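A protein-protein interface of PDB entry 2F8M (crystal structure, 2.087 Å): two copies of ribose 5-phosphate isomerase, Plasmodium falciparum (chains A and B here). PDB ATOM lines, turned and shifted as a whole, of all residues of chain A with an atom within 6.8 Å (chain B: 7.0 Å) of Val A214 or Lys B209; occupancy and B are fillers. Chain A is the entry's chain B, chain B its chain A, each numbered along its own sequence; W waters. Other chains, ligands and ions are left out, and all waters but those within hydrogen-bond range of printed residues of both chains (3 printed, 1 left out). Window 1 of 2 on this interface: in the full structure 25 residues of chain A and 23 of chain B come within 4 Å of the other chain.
Of the 19 printed residues of chain B, 8 touch a printed residue of chain A.
Hydrophobic or aromatic side chains of chain B that line the printed part of chain A: Leu B116 and Met B210.
Hydrophobic or aromatic side chains of chain A that line the printed part of chain B: Ile A156 and Met A210.
Among the printed residues, 13 pairs touch across the chains.
Among the printed residues, no Asp or Glu carboxylate lies within 4 Å of a Lys or Arg side-chain nitrogen of the other chain.
Of chain A, only Lys A209, Met A210, Thr A211 and Val A214 come within 4 Å of Lys B209.
No residue of chain B comes within 4 Å of Gly A213.
Of the printed residues of chain B, Asp A216 touches Thr B212 (3.6 Å).
Of the printed residues of chain A, Met B210 touches Lys A209 and Met A210.
Leu A160 touches none of the printed residues of chain B.
Ile B163 touches none of the printed residues of chain A.
The nearest residue of chain A that does not touch Lys B209 is Thr A212 (4.3 Å).
The nearest printed residue of chain A that does not touch Val B214 is Val A215 (4.05 Å).
Among the printed residues, pairs that only touch across the chains: Ile A156 with Leu B116 (3.9 Å), Lys A209 with Met B210 (3.8 Å), Met A210 with Thr B206 (3.96 Å), Met A210 with Lys B209 (3.8 Å), Thr A212 with Leu B116 (3.8 Å), Thr A212 with Asp B216 (3.8 Å) and Asp A216 with Thr B212 (3.6 Å).
The side-chain amino group (NZ) of Lys B209 lies within hydrogen-bond range of the backbone carbonyl oxygen (O) of Thr A211 (2.9 Å).
O of Lys A209 lies within hydrogen-bond range of NZ of Lys B209 (2.6 Å).
O of Val B214 lies within hydrogen-bond range of NZ of Lys A209 (3.4 Å).
The side-chain amino group (NZ) of Lys B209 sits at hydrogen-bond distance from the backbone carbonyl oxygen (O) of Val A214.
NZ of Lys A209 lies within hydrogen-bond range of O of Thr B211, 2.9 Å away.
SD of Met B210 sits close to SD of Met A210.
Water W2 lies within hydrogen-bond range of the side-chain carboxylate (OD2) of Asp B216 and the side-chain hydroxyl (OG1) of Thr A212.
Water W3 bridges OD2 of Asp A216 (2.6 Å) and OG1 of Thr B212 (2.7 Å).
Water W1 lies within hydrogen-bond range of the backbone NH of Gly A213, the backbone carbonyl oxygen of Val B215 and the side-chain carboxylate of Asp B216.
O of Arg A207 sits at hydrogen-bond distance from OG1 of Thr A211 (2.7 Å).
The side-chain hydroxyl (OG1) of Thr A211 sits close to the backbone carbonyl oxygen (O) of Ile A208 (3.1 Å).
The side-chain hydroxyl of Thr B211 lies close to the backbone carbonyl oxygen of Ile B208 (3.4 Å).
The side-chain hydroxyl (OG1) of Thr B211 sits at hydrogen-bond distance from the backbone carbonyl oxygen (O) of Arg B207 (2.8 Å).
The backbone carbonyl oxygen (O) of Asp A216 lies within hydrogen-bond range of the backbone NH (N) of Glu A147, at 2.7 Å.
The side-chain amino group (NZ) of Lys B115 is in salt-bridge range of the side-chain carboxylate (OD1) of Asp B216 (2.5 Å).
Lys A209 touches its own counterpart, Lys B209.
Lys A209 touches Met B210, and with the chains exchanged Met A210 touches Lys B209.
Lys A209 touches Val B214, and with the chains exchanged Val A214 touches Lys B209.
Thr A212 touches Asp B216, and with the chains exchanged Asp A216 touches Thr B212.
12 positions are printed for both chains.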
ATOM      1  N   ILE A 146     -16.233 -11.214   8.896  1.00  0.00           N
ATOM      2  CA  ILE A 146     -16.874  -9.953   8.472  1.00  0.00           C
ATOM      3  C   ILE A 146     -18.329 -10.098   8.803  1.00  0.00           C
ATOM      4  O   ILE A 146     -18.992 -11.053   8.349  1.00  0.00           O
ATOM      5  CB  ILE A 146     -16.644  -9.598   6.990  1.00  0.00           C
ATOM      6  CG1 ILE A 146     -15.154  -9.420   6.682  1.00  0.00           C
ATOM      7  CG2 ILE A 146     -17.331  -8.288   6.656  1.00  0.00           C
ATOM      8  CD1 ILE A 146     -14.842  -9.388   5.157  1.00  0.00           C
ATOM      9  N   GLU A 147     -18.793  -9.242   9.707  1.00  0.00           N
ATOM     10  CA  GLU A 147     -20.184  -9.283  10.091  1.00  0.00           C
ATOM     11  C   GLU A 147     -21.037  -8.516   9.035  1.00  0.00           C
ATOM     12  O   GLU A 147     -20.706  -7.370   8.644  1.00  0.00           O
ATOM     13  CB  GLU A 147     -20.399  -8.761  11.524  1.00  0.00           C
ATOM     14  CG  GLU A 147     -21.795  -9.066  12.033  1.00  0.00           C
ATOM     15  CD  GLU A 147     -21.962  -9.062  13.545  1.00  0.00           C
ATOM     16  OE1 GLU A 147     -21.002  -9.465  14.300  1.00  0.00           O
ATOM     17  OE2 GLU A 147     -23.099  -8.686  13.981  1.00  0.00           O
ATOM     18  N   ILE A 148     -22.114  -9.169   8.590  1.00  0.00           N
ATOM     19  CA  ILE A 148     -22.930  -8.672   7.515  1.00  0.00           C
ATOM     20  C   ILE A 148     -24.424  -8.930   7.760  1.00  0.00           C
ATOM     21  O   ILE A 148     -24.791  -9.777   8.587  1.00  0.00           O
ATOM     22  CB  ILE A 148     -22.489  -9.276   6.129  1.00  0.00           C
ATOM     23  CG1 ILE A 148     -22.486 -10.794   6.171  1.00  0.00           C
ATOM     24  CG2 ILE A 148     -21.127  -8.851   5.807  1.00  0.00           C
ATOM     25  CD1 ILE A 148     -22.444 -11.474   4.786  1.00  0.00           C
ATOM     26  N   LEU A 149     -25.283  -8.194   7.014  1.00  0.00           N
ATOM     27  CA  LEU A 149     -26.719  -8.340   7.155  1.00  0.00           C
ATOM     28  C   LEU A 149     -27.121  -9.670   6.660  1.00  0.00           C
ATOM     29  O   LEU A 149     -26.516 -10.186   5.770  1.00  0.00           O
ATOM     30  CB  LEU A 149     -27.520  -7.320   6.302  1.00  0.00           C
ATOM     31  CG  LEU A 149     -27.326  -5.807   6.410  1.00  0.00           C
ATOM     32  CD1 LEU A 149     -28.292  -5.149   5.437  1.00  0.00           C
ATOM     33  CD2 LEU A 149     -27.519  -5.269   7.816  1.00  0.00           C
ATOM     34  N   ILE A 156     -23.807  -8.822  -0.528  1.00  0.00           N
ATOM     35  CA  ILE A 156     -22.758  -8.196   0.251  1.00  0.00           C
ATOM     36  C   ILE A 156     -21.442  -8.970   0.048  1.00  0.00           C
ATOM     37  O   ILE A 156     -20.368  -8.361  -0.184  1.00  0.00           O
ATOM     38  CB  ILE A 156     -23.159  -8.096   1.706  1.00  0.00           C
ATOM     39  CG1 ILE A 156     -24.466  -7.303   1.809  1.00  0.00           C
ATOM     40  CG2 ILE A 156     -22.023  -7.445   2.583  1.00  0.00           C
ATOM     41  CD1 ILE A 156     -25.160  -7.455   3.206  1.00  0.00           C
ATOM     42  N   LEU A 160     -17.910  -7.535  -1.349  1.00  0.00           N
ATOM     43  CA  LEU A 160     -16.634  -7.698  -0.618  1.00  0.00           C
ATOM     44  C   LEU A 160     -15.550  -8.273  -1.505  1.00  0.00           C
ATOM     45  O   LEU A 160     -14.362  -7.930  -1.371  1.00  0.00           O
ATOM     46  CB  LEU A 160     -16.825  -8.566   0.605  1.00  0.00           C
ATOM     47  CG  LEU A 160     -17.477  -7.858   1.799  1.00  0.00           C
ATOM     48  CD1 LEU A 160     -17.902  -8.864   2.839  1.00  0.00           C
ATOM     49  CD2 LEU A 160     -16.558  -6.819   2.434  1.00  0.00           C
ATOM     50  N   ARG A 207     -12.043  -0.445   3.588  1.00  0.00           N
ATOM     51  CA  ARG A 207     -12.870  -0.765   2.441  1.00  0.00           C
ATOM     52  C   ARG A 207     -13.931  -1.763   2.828  1.00  0.00           C
ATOM     53  O   ARG A 207     -15.031  -1.724   2.288  1.00  0.00           O
ATOM     54  CB  ARG A 207     -12.011  -1.325   1.309  1.00  0.00           C
ATOM     55  CG  ARG A 207     -11.246  -0.263   0.529  1.00  0.00           C
ATOM     56  CD  ARG A 207      -9.969  -0.818  -0.058  1.00  0.00           C
ATOM     57  NE  ARG A 207      -9.232   0.151  -0.879  1.00  0.00           N
ATOM     58  CZ  ARG A 207      -9.508   0.426  -2.159  1.00  0.00           C
ATOM     59  NH1 ARG A 207     -10.518  -0.183  -2.800  1.00  0.00           N
ATOM     60  NH2 ARG A 207      -8.760   1.308  -2.796  1.00  0.00           N
ATOM     61  N   ILE A 208     -13.627  -2.636   3.788  1.00  0.00           N
ATOM     62  CA  ILE A 208     -14.640  -3.527   4.314  1.00  0.00           C
ATOM     63  C   ILE A 208     -15.702  -2.706   5.032  1.00  0.00           C
ATOM     64  O   ILE A 208     -16.875  -2.767   4.657  1.00  0.00           O
ATOM     65  CB  ILE A 208     -14.040  -4.604   5.247  1.00  0.00           C
ATOM     66  CG1 ILE A 208     -13.115  -5.497   4.447  1.00  0.00           C
ATOM     67  CG2 ILE A 208     -15.137  -5.425   5.880  1.00  0.00           C
ATOM     68  CD1 ILE A 208     -12.244  -6.451   5.282  1.00  0.00           C
ATOM     69  N   LYS A 209     -15.263  -1.929   6.032  1.00  0.00           N
ATOM     70  CA  LYS A 209     -16.127  -1.087   6.842  1.00  0.00           C
ATOM     71  C   LYS A 209     -17.053  -0.162   6.044  1.00  0.00           C
ATOM     72  O   LYS A 209     -18.199   0.070   6.452  1.00  0.00           O
ATOM     73  CB  LYS A 209     -15.309  -0.236   7.830  1.00  0.00           C
ATOM     74  CG  LYS A 209     -16.162   0.516   8.863  1.00  0.00           C
ATOM     75  CD  LYS A 209     -17.051  -0.472   9.637  1.00  0.00           C
ATOM     76  CE  LYS A 209     -17.647   0.122  10.952  1.00  0.00           C
ATOM     77  NZ  LYS A 209     -18.950   0.775  10.712  1.00  0.00           N
ATOM     78  N   MET A 210     -16.576   0.293   4.892  1.00  0.00           N
ATOM     79  CA  MET A 210     -17.311   1.218   4.041  1.00  0.00           C
ATOM     80  C   MET A 210     -18.280   0.505   3.148  1.00  0.00           C
ATOM     81  O   MET A 210     -19.121   1.135   2.502  1.00  0.00           O
ATOM     82  CB  MET A 210     -16.321   1.998   3.163  1.00  0.00           C
ATOM     83  CG  MET A 210     -15.494   3.003   3.925  1.00  0.00           C
ATOM     84  SD  MET A 210     -16.536   4.313   4.610  1.00  0.00           S
ATOM     85  CE  MET A 210     -17.278   5.013   3.131  1.00  0.00           C
ATOM     86  N   THR A 211     -18.183  -0.820   3.119  1.00  0.00           N
ATOM     87  CA  THR A 211     -19.105  -1.614   2.340  1.00  0.00           C
ATOM     88  C   THR A 211     -20.589  -1.608   2.877  1.00  0.00           C
ATOM     89  O   THR A 211     -20.896  -1.895   4.037  1.00  0.00           O
ATOM     90  CB  THR A 211     -18.595  -3.074   2.183  1.00  0.00           C
ATOM     91  OG1 THR A 211     -17.283  -3.078   1.620  1.00  0.00           O
ATOM     92  CG2 THR A 211     -19.514  -3.873   1.268  1.00  0.00           C
ATOM     93  N   THR A 212     -21.499  -1.286   1.952  1.00  0.00           N
ATOM     94  CA  THR A 212     -22.899  -1.253   2.249  1.00  0.00           C
ATOM     95  C   THR A 212     -23.287  -2.688   2.621  1.00  0.00           C
ATOM     96  O   THR A 212     -23.021  -3.625   1.858  1.00  0.00           O
ATOM     97  CB  THR A 212     -23.743  -0.662   1.019  1.00  0.00           C
ATOM     98  OG1 THR A 212     -23.254   0.633   0.645  1.00  0.00           O
ATOM     99  CG2 THR A 212     -25.205  -0.565   1.367  1.00  0.00           C
ATOM    100  N   GLY A 213     -23.889  -2.846   3.802  1.00  0.00           N
ATOM    101  CA  GLY A 213     -24.296  -4.147   4.348  1.00  0.00           C
ATOM    102  C   GLY A 213     -23.285  -4.780   5.331  1.00  0.00           C
ATOM    103  O   GLY A 213     -23.566  -5.815   5.931  1.00  0.00           O
ATOM    104  N   VAL A 214     -22.095  -4.182   5.445  1.00  0.00           N
ATOM    105  CA  VAL A 214     -21.137  -4.629   6.427  1.00  0.00           C
ATOM    106  C   VAL A 214     -21.363  -3.867   7.718  1.00  0.00           C
ATOM    107  O   VAL A 214     -21.449  -2.648   7.717  1.00  0.00           O
ATOM    108  CB  VAL A 214     -19.698  -4.456   5.966  1.00  0.00           C
ATOM    109  CG1 VAL A 214     -18.749  -4.706   7.149  1.00  0.00           C
ATOM    110  CG2 VAL A 214     -19.362  -5.432   4.840  1.00  0.00           C
ATOM    111  N   VAL A 215     -21.446  -4.612   8.815  1.00  0.00           N
ATOM    112  CA  VAL A 215     -21.567  -4.041  10.151  1.00  0.00           C
ATOM    113  C   VAL A 215     -20.191  -3.757  10.747  1.00  0.00           C
ATOM    114  O   VAL A 215     -19.891  -2.617  11.082  1.00  0.00           O
ATOM    115  CB  VAL A 215     -22.350  -4.943  11.083  1.00  0.00           C
ATOM    116  CG1 VAL A 215     -22.448  -4.279  12.442  1.00  0.00           C
ATOM    117  CG2 VAL A 215     -23.732  -5.259  10.445  1.00  0.00           C
ATOM    118  N   ASP A 216     -19.357  -4.773  10.869  1.00  0.00           N
ATOM    119  CA  ASP A 216     -17.952  -4.567  11.176  1.00  0.00           C
ATOM    120  C   ASP A 216     -17.225  -5.856  10.842  1.00  0.00           C
ATOM    121  O   ASP A 216     -17.817  -6.778  10.274  1.00  0.00           O
ATOM    122  CB  ASP A 216     -17.690  -4.164  12.648  1.00  0.00           C
ATOM    123  CG  ASP A 216     -16.512  -3.126  12.806  1.00  0.00           C
ATOM    124  OD1 ASP A 216     -15.411  -3.294  12.200  1.00  0.00           O
ATOM    125  OD2 ASP A 216     -16.688  -2.129  13.555  1.00  0.00           O
ATOM    126  N   HIS A 217     -15.924  -5.858  11.123  1.00  0.00           N
ATOM    127  CA  HIS A 217     -15.013  -6.922  10.751  1.00  0.00           C
ATOM    128  C   HIS A 217     -14.114  -7.163  11.936  1.00  0.00           C
ATOM    129  O   HIS A 217     -14.020  -6.312  12.848  1.00  0.00           O
ATOM    130  CB  HIS A 217     -14.168  -6.556   9.539  1.00  0.00           C
ATOM    131  CG  HIS A 217     -13.361  -5.310   9.717  1.00  0.00           C
ATOM    132  ND1 HIS A 217     -12.105  -5.308  10.279  1.00  0.00           N
ATOM    133  CD2 HIS A 217     -13.607  -4.022   9.352  1.00  0.00           C
ATOM    134  CE1 HIS A 217     -11.643  -4.067  10.315  1.00  0.00           C
ATOM    135  NE2 HIS A 217     -12.523  -3.273   9.736  1.00  0.00           N
ATOM    136  N   LYS B 115     -30.499   1.352   0.503  1.00  0.00           N
ATOM    137  CA  LYS B 115     -29.181   1.641  -0.101  1.00  0.00           C
ATOM    138  C   LYS B 115     -28.593   0.390  -0.765  1.00  0.00           C
ATOM    139  O   LYS B 115     -28.015   0.447  -1.865  1.00  0.00           O
ATOM    140  CB  LYS B 115     -28.202   2.207   0.923  1.00  0.00           C
ATOM    141  CG  LYS B 115     -27.019   2.961   0.314  1.00  0.00           C
ATOM    142  CD  LYS B 115     -26.127   3.553   1.402  1.00  0.00           C
ATOM    143  CE  LYS B 115     -26.618   4.939   1.968  1.00  0.00           C
ATOM    144  NZ  LYS B 115     -25.674   5.535   2.965  1.00  0.00           N
ATOM    145  N   LEU B 116     -28.753  -0.745  -0.118  1.00  0.00           N
ATOM    146  CA  LEU B 116     -28.191  -1.977  -0.658  1.00  0.00           C
ATOM    147  C   LEU B 116     -28.813  -2.375  -1.975  1.00  0.00           C
ATOM    148  O   LEU B 116     -28.130  -2.682  -2.927  1.00  0.00           O
ATOM    149  CB  LEU B 116     -28.376  -3.114   0.348  1.00  0.00           C
ATOM    150  CG  LEU B 116     -27.675  -4.446  -0.004  1.00  0.00           C
ATOM    151  CD1 LEU B 116     -26.153  -4.335  -0.121  1.00  0.00           C
ATOM    152  CD2 LEU B 116     -28.017  -5.478   1.047  1.00  0.00           C
ATOM    153  N   ILE B 146     -29.668   7.542  11.060  1.00  0.00           N
ATOM    154  CA  ILE B 146     -28.475   6.716  11.112  1.00  0.00           C
ATOM    155  C   ILE B 146     -28.869   5.466  11.893  1.00  0.00           C
ATOM    156  O   ILE B 146     -29.412   5.552  13.001  1.00  0.00           O
ATOM    157  CB  ILE B 146     -27.270   7.450  11.760  1.00  0.00           C
ATOM    158  CG1 ILE B 146     -27.056   8.818  11.137  1.00  0.00           C
ATOM    159  CG2 ILE B 146     -25.961   6.627  11.620  1.00  0.00           C
ATOM    160  CD1 ILE B 146     -25.979   9.646  11.795  1.00  0.00           C
ATOM    161  N   LEU B 160     -20.725   9.605  17.452  1.00  0.00           N
ATOM    162  CA  LEU B 160     -21.155  10.345  16.249  1.00  0.00           C
ATOM    163  C   LEU B 160     -21.040  11.851  16.436  1.00  0.00           C
ATOM    164  O   LEU B 160     -20.660  12.591  15.536  1.00  0.00           O
ATOM    165  CB  LEU B 160     -22.594   9.968  15.860  1.00  0.00           C
ATOM    166  CG  LEU B 160     -22.709   8.620  15.141  1.00  0.00           C
ATOM    167  CD1 LEU B 160     -24.107   8.037  15.273  1.00  0.00           C
ATOM    168  CD2 LEU B 160     -22.337   8.774  13.697  1.00  0.00           C
ATOM    169  N   ILE B 163     -17.903  13.828  15.308  1.00  0.00           N
ATOM    170  CA  ILE B 163     -17.674  14.139  13.907  1.00  0.00           C
ATOM    171  C   ILE B 163     -17.895  15.634  13.752  1.00  0.00           C
ATOM    172  O   ILE B 163     -18.948  16.174  14.123  1.00  0.00           O
ATOM    173  CB  ILE B 163     -18.606  13.347  12.999  1.00  0.00           C
ATOM    174  CG1 ILE B 163     -18.326  11.851  13.129  1.00  0.00           C
ATOM    175  CG2 ILE B 163     -18.495  13.794  11.535  1.00  0.00           C
ATOM    176  CD1 ILE B 163     -19.325  11.003  12.337  1.00  0.00           C
ATOM    177  N   GLU B 203     -17.655  13.720   3.032  1.00  0.00           N
ATOM    178  CA  GLU B 203     -16.811  13.428   4.177  1.00  0.00           C
ATOM    179  C   GLU B 203     -17.617  12.981   5.377  1.00  0.00           C
ATOM    180  O   GLU B 203     -17.216  12.083   6.083  1.00  0.00           O
ATOM    181  CB  GLU B 203     -15.948  14.634   4.555  1.00  0.00           C
ATOM    182  CG  GLU B 203     -14.904  14.333   5.633  1.00  0.00           C
ATOM    183  CD  GLU B 203     -13.858  13.207   5.278  1.00  0.00           C
ATOM    184  OE1 GLU B 203     -13.620  12.953   4.068  1.00  0.00           O
ATOM    185  OE2 GLU B 203     -13.289  12.573   6.226  1.00  0.00           O
ATOM    186  N   THR B 204     -18.748  13.643   5.598  1.00  0.00           N
ATOM    187  CA  THR B 204     -19.709  13.281   6.651  1.00  0.00           C
ATOM    188  C   THR B 204     -20.181  11.833   6.497  1.00  0.00           C
ATOM    189  O   THR B 204     -20.145  11.080   7.460  1.00  0.00           O
ATOM    190  CB  THR B 204     -20.920  14.277   6.641  1.00  0.00           C
ATOM    191  OG1 THR B 204     -20.452  15.608   6.930  1.00  0.00           O
ATOM    192  CG2 THR B 204     -21.947  13.905   7.647  1.00  0.00           C
ATOM    193  N   CYS B 205     -20.589  11.450   5.294  1.00  0.00           N
ATOM    194  CA  CYS B 205     -21.092  10.070   4.995  1.00  0.00           C
ATOM    195  C   CYS B 205     -20.031   9.051   5.361  1.00  0.00           C
ATOM    196  O   CYS B 205     -20.259   8.093   6.047  1.00  0.00           O
ATOM    197  CB  CYS B 205     -21.425   9.893   3.516  1.00  0.00           C
ATOM    198  SG  CYS B 205     -22.779  10.850   2.895  1.00  0.00           S
ATOM    199  N   THR B 206     -18.830   9.350   4.921  1.00  0.00           N
ATOM    200  CA  THR B 206     -17.662   8.521   5.151  1.00  0.00           C
ATOM    201  C   THR B 206     -17.381   8.412   6.628  1.00  0.00           C
ATOM    202  O   THR B 206     -17.231   7.324   7.104  1.00  0.00           O
ATOM    203  CB  THR B 206     -16.466   9.087   4.370  1.00  0.00           C
ATOM    204  OG1 THR B 206     -16.741   8.933   2.962  1.00  0.00           O
ATOM    205  CG2 THR B 206     -15.166   8.348   4.731  1.00  0.00           C
ATOM    206  N   ARG B 207     -17.377   9.522   7.365  1.00  0.00           N
ATOM    207  CA  ARG B 207     -17.099   9.448   8.828  1.00  0.00           C
ATOM    208  C   ARG B 207     -18.218   8.773   9.651  1.00  0.00           C
ATOM    209  O   ARG B 207     -17.973   8.125  10.695  1.00  0.00           O
ATOM    210  CB  ARG B 207     -16.757  10.846   9.372  1.00  0.00           C
ATOM    211  CG  ARG B 207     -15.419  11.374   8.941  1.00  0.00           C
ATOM    212  CD  ARG B 207     -15.324  12.845   9.299  1.00  0.00           C
ATOM    213  NE  ARG B 207     -14.158  13.527   8.708  1.00  0.00           N
ATOM    214  CZ  ARG B 207     -13.097  13.981   9.379  1.00  0.00           C
ATOM    215  NH1 ARG B 207     -13.007  13.833  10.703  1.00  0.00           N
ATOM    216  NH2 ARG B 207     -12.124  14.592   8.707  1.00  0.00           N
ATOM    217  N   ILE B 208     -19.450   8.905   9.184  1.00  0.00           N
ATOM    218  CA  ILE B 208     -20.549   8.221   9.821  1.00  0.00           C
ATOM    219  C   ILE B 208     -20.401   6.700   9.607  1.00  0.00           C
ATOM    220  O   ILE B 208     -20.514   5.889  10.517  1.00  0.00           O
ATOM    221  CB  ILE B 208     -21.913   8.675   9.244  1.00  0.00           C
ATOM    222  CG1 ILE B 208     -22.246  10.094   9.662  1.00  0.00           C
ATOM    223  CG2 ILE B 208     -22.994   7.719   9.727  1.00  0.00           C
ATOM    224  CD1 ILE B 208     -23.426  10.709   8.965  1.00  0.00           C
ATOM    225  N   LYS B 209     -20.155   6.337   8.364  1.00  0.00           N
ATOM    226  CA  LYS B 209     -20.111   4.953   7.986  1.00  0.00           C
ATOM    227  C   LYS B 209     -18.955   4.248   8.607  1.00  0.00           C
ATOM    228  O   LYS B 209     -19.085   3.065   8.865  1.00  0.00           O
ATOM    229  CB  LYS B 209     -20.004   4.793   6.471  1.00  0.00           C
ATOM    230  CG  LYS B 209     -20.013   3.339   5.987  1.00  0.00           C
ATOM    231  CD  LYS B 209     -21.371   2.640   6.248  1.00  0.00           C
ATOM    232  CE  LYS B 209     -21.550   1.304   5.466  1.00  0.00           C
ATOM    233  NZ  LYS B 209     -20.723   0.212   6.018  1.00  0.00           N
ATOM    234  N   MET B 210     -17.836   4.951   8.785  1.00  0.00           N
ATOM    235  CA  MET B 210     -16.628   4.404   9.438  1.00  0.00           C
ATOM    236  C   MET B 210     -16.813   4.214  10.938  1.00  0.00           C
ATOM    237  O   MET B 210     -16.015   3.517  11.584  1.00  0.00           O
ATOM    238  CB  MET B 210     -15.421   5.325   9.184  1.00  0.00           C
ATOM    239  CG  MET B 210     -14.892   5.273   7.751  1.00  0.00           C
ATOM    240  SD  MET B 210     -14.434   3.573   7.224  1.00  0.00           S
ATOM    241  CE  MET B 210     -13.014   3.304   8.322  1.00  0.00           C
ATOM    242  N   THR B 211     -17.885   4.756  11.496  1.00  0.00           N
ATOM    243  CA  THR B 211     -18.104   4.660  12.967  1.00  0.00           C
ATOM    244  C   THR B 211     -18.464   3.243  13.456  1.00  0.00           C
ATOM    245  O   THR B 211     -19.348   2.572  12.935  1.00  0.00           O
ATOM    246  CB  THR B 211     -19.179   5.688  13.441  1.00  0.00           C
ATOM    247  OG1 THR B 211     -18.725   7.027  13.170  1.00  0.00           O
ATOM    248  CG2 THR B 211     -19.435   5.583  14.910  1.00  0.00           C
ATOM    249  N   THR B 212     -17.773   2.790  14.502  1.00  0.00           N
ATOM    250  CA  THR B 212     -18.121   1.524  15.121  1.00  0.00           C
ATOM    251  C   THR B 212     -19.504   1.596  15.710  1.00  0.00           C
ATOM    252  O   THR B 212     -19.828   2.468  16.498  1.00  0.00           O
ATOM    253  CB  THR B 212     -17.087   1.130  16.226  1.00  0.00           C
ATOM    254  OG1 THR B 212     -15.771   1.293  15.691  1.00  0.00           O
ATOM    255  CG2 THR B 212     -17.292  -0.280  16.643  1.00  0.00           C
ATOM    256  N   VAL B 214     -22.209   1.885  13.755  1.00  0.00           N
ATOM    257  CA  VAL B 214     -23.072   2.392  12.672  1.00  0.00           C
ATOM    258  C   VAL B 214     -23.239   1.276  11.634  1.00  0.00           C
ATOM    259  O   VAL B 214     -22.267   0.657  11.215  1.00  0.00           O
ATOM    260  CB  VAL B 214     -22.515   3.722  12.062  1.00  0.00           C
ATOM    261  CG1 VAL B 214     -23.265   4.176  10.829  1.00  0.00           C
ATOM    262  CG2 VAL B 214     -22.547   4.867  13.106  1.00  0.00           C
ATOM    263  N   VAL B 215     -24.497   0.986  11.273  1.00  0.00           N
ATOM    264  CA  VAL B 215     -24.782   0.071  10.199  1.00  0.00           C
ATOM    265  C   VAL B 215     -24.741   0.855   8.861  1.00  0.00           C
ATOM    266  O   VAL B 215     -23.929   0.555   7.978  1.00  0.00           O
ATOM    267  CB  VAL B 215     -26.113  -0.610  10.431  1.00  0.00           C
ATOM    268  CG1 VAL B 215     -26.469  -1.490   9.217  1.00  0.00           C
ATOM    269  CG2 VAL B 215     -26.028  -1.400  11.707  1.00  0.00           C
ATOM    270  N   ASP B 216     -25.591   1.871   8.752  1.00  0.00           N
ATOM    271  CA  ASP B 216     -25.536   2.826   7.636  1.00  0.00           C
ATOM    272  C   ASP B 216     -26.341   4.061   8.014  1.00  0.00           C
ATOM    273  O   ASP B 216     -26.901   4.155   9.135  1.00  0.00           O
ATOM    274  CB  ASP B 216     -26.063   2.217   6.308  1.00  0.00           C
ATOM    275  CG  ASP B 216     -25.215   2.664   5.044  1.00  0.00           C
ATOM    276  OD1 ASP B 216     -25.054   3.909   4.808  1.00  0.00           O
ATOM    277  OD2 ASP B 216     -24.735   1.774   4.274  1.00  0.00           O
ATOM    278  N   HIS B 217     -26.354   5.025   7.102  1.00  0.00           N
ATOM    279  CA  HIS B 217     -27.062   6.273   7.311  1.00  0.00           C
ATOM    280  C   HIS B 217     -27.926   6.574   6.089  1.00  0.00           C
ATOM    281  O   HIS B 217     -27.729   5.991   4.991  1.00  0.00           O
ATOM    282  CB  HIS B 217     -26.072   7.410   7.514  1.00  0.00           C
ATOM    283  CG  HIS B 217     -25.006   7.466   6.465  1.00  0.00           C
ATOM    284  ND1 HIS B 217     -25.187   8.117   5.260  1.00  0.00           N
ATOM    285  CD2 HIS B 217     -23.778   6.891   6.409  1.00  0.00           C
ATOM    286  CE1 HIS B 217     -24.104   7.962   4.526  1.00  0.00           C
ATOM    287  NE2 HIS B 217     -23.226   7.247   5.208  1.00  0.00           N
HETATM  288  O   HOH W   1     -24.471  -0.836   5.526  1.00  0.00           O
HETATM  289  O   HOH W   2     -23.111   2.469   2.459  1.00  0.00           O
HETATM  290  O   HOH W   3     -15.183  -0.022  13.417  1.00  0.00           O
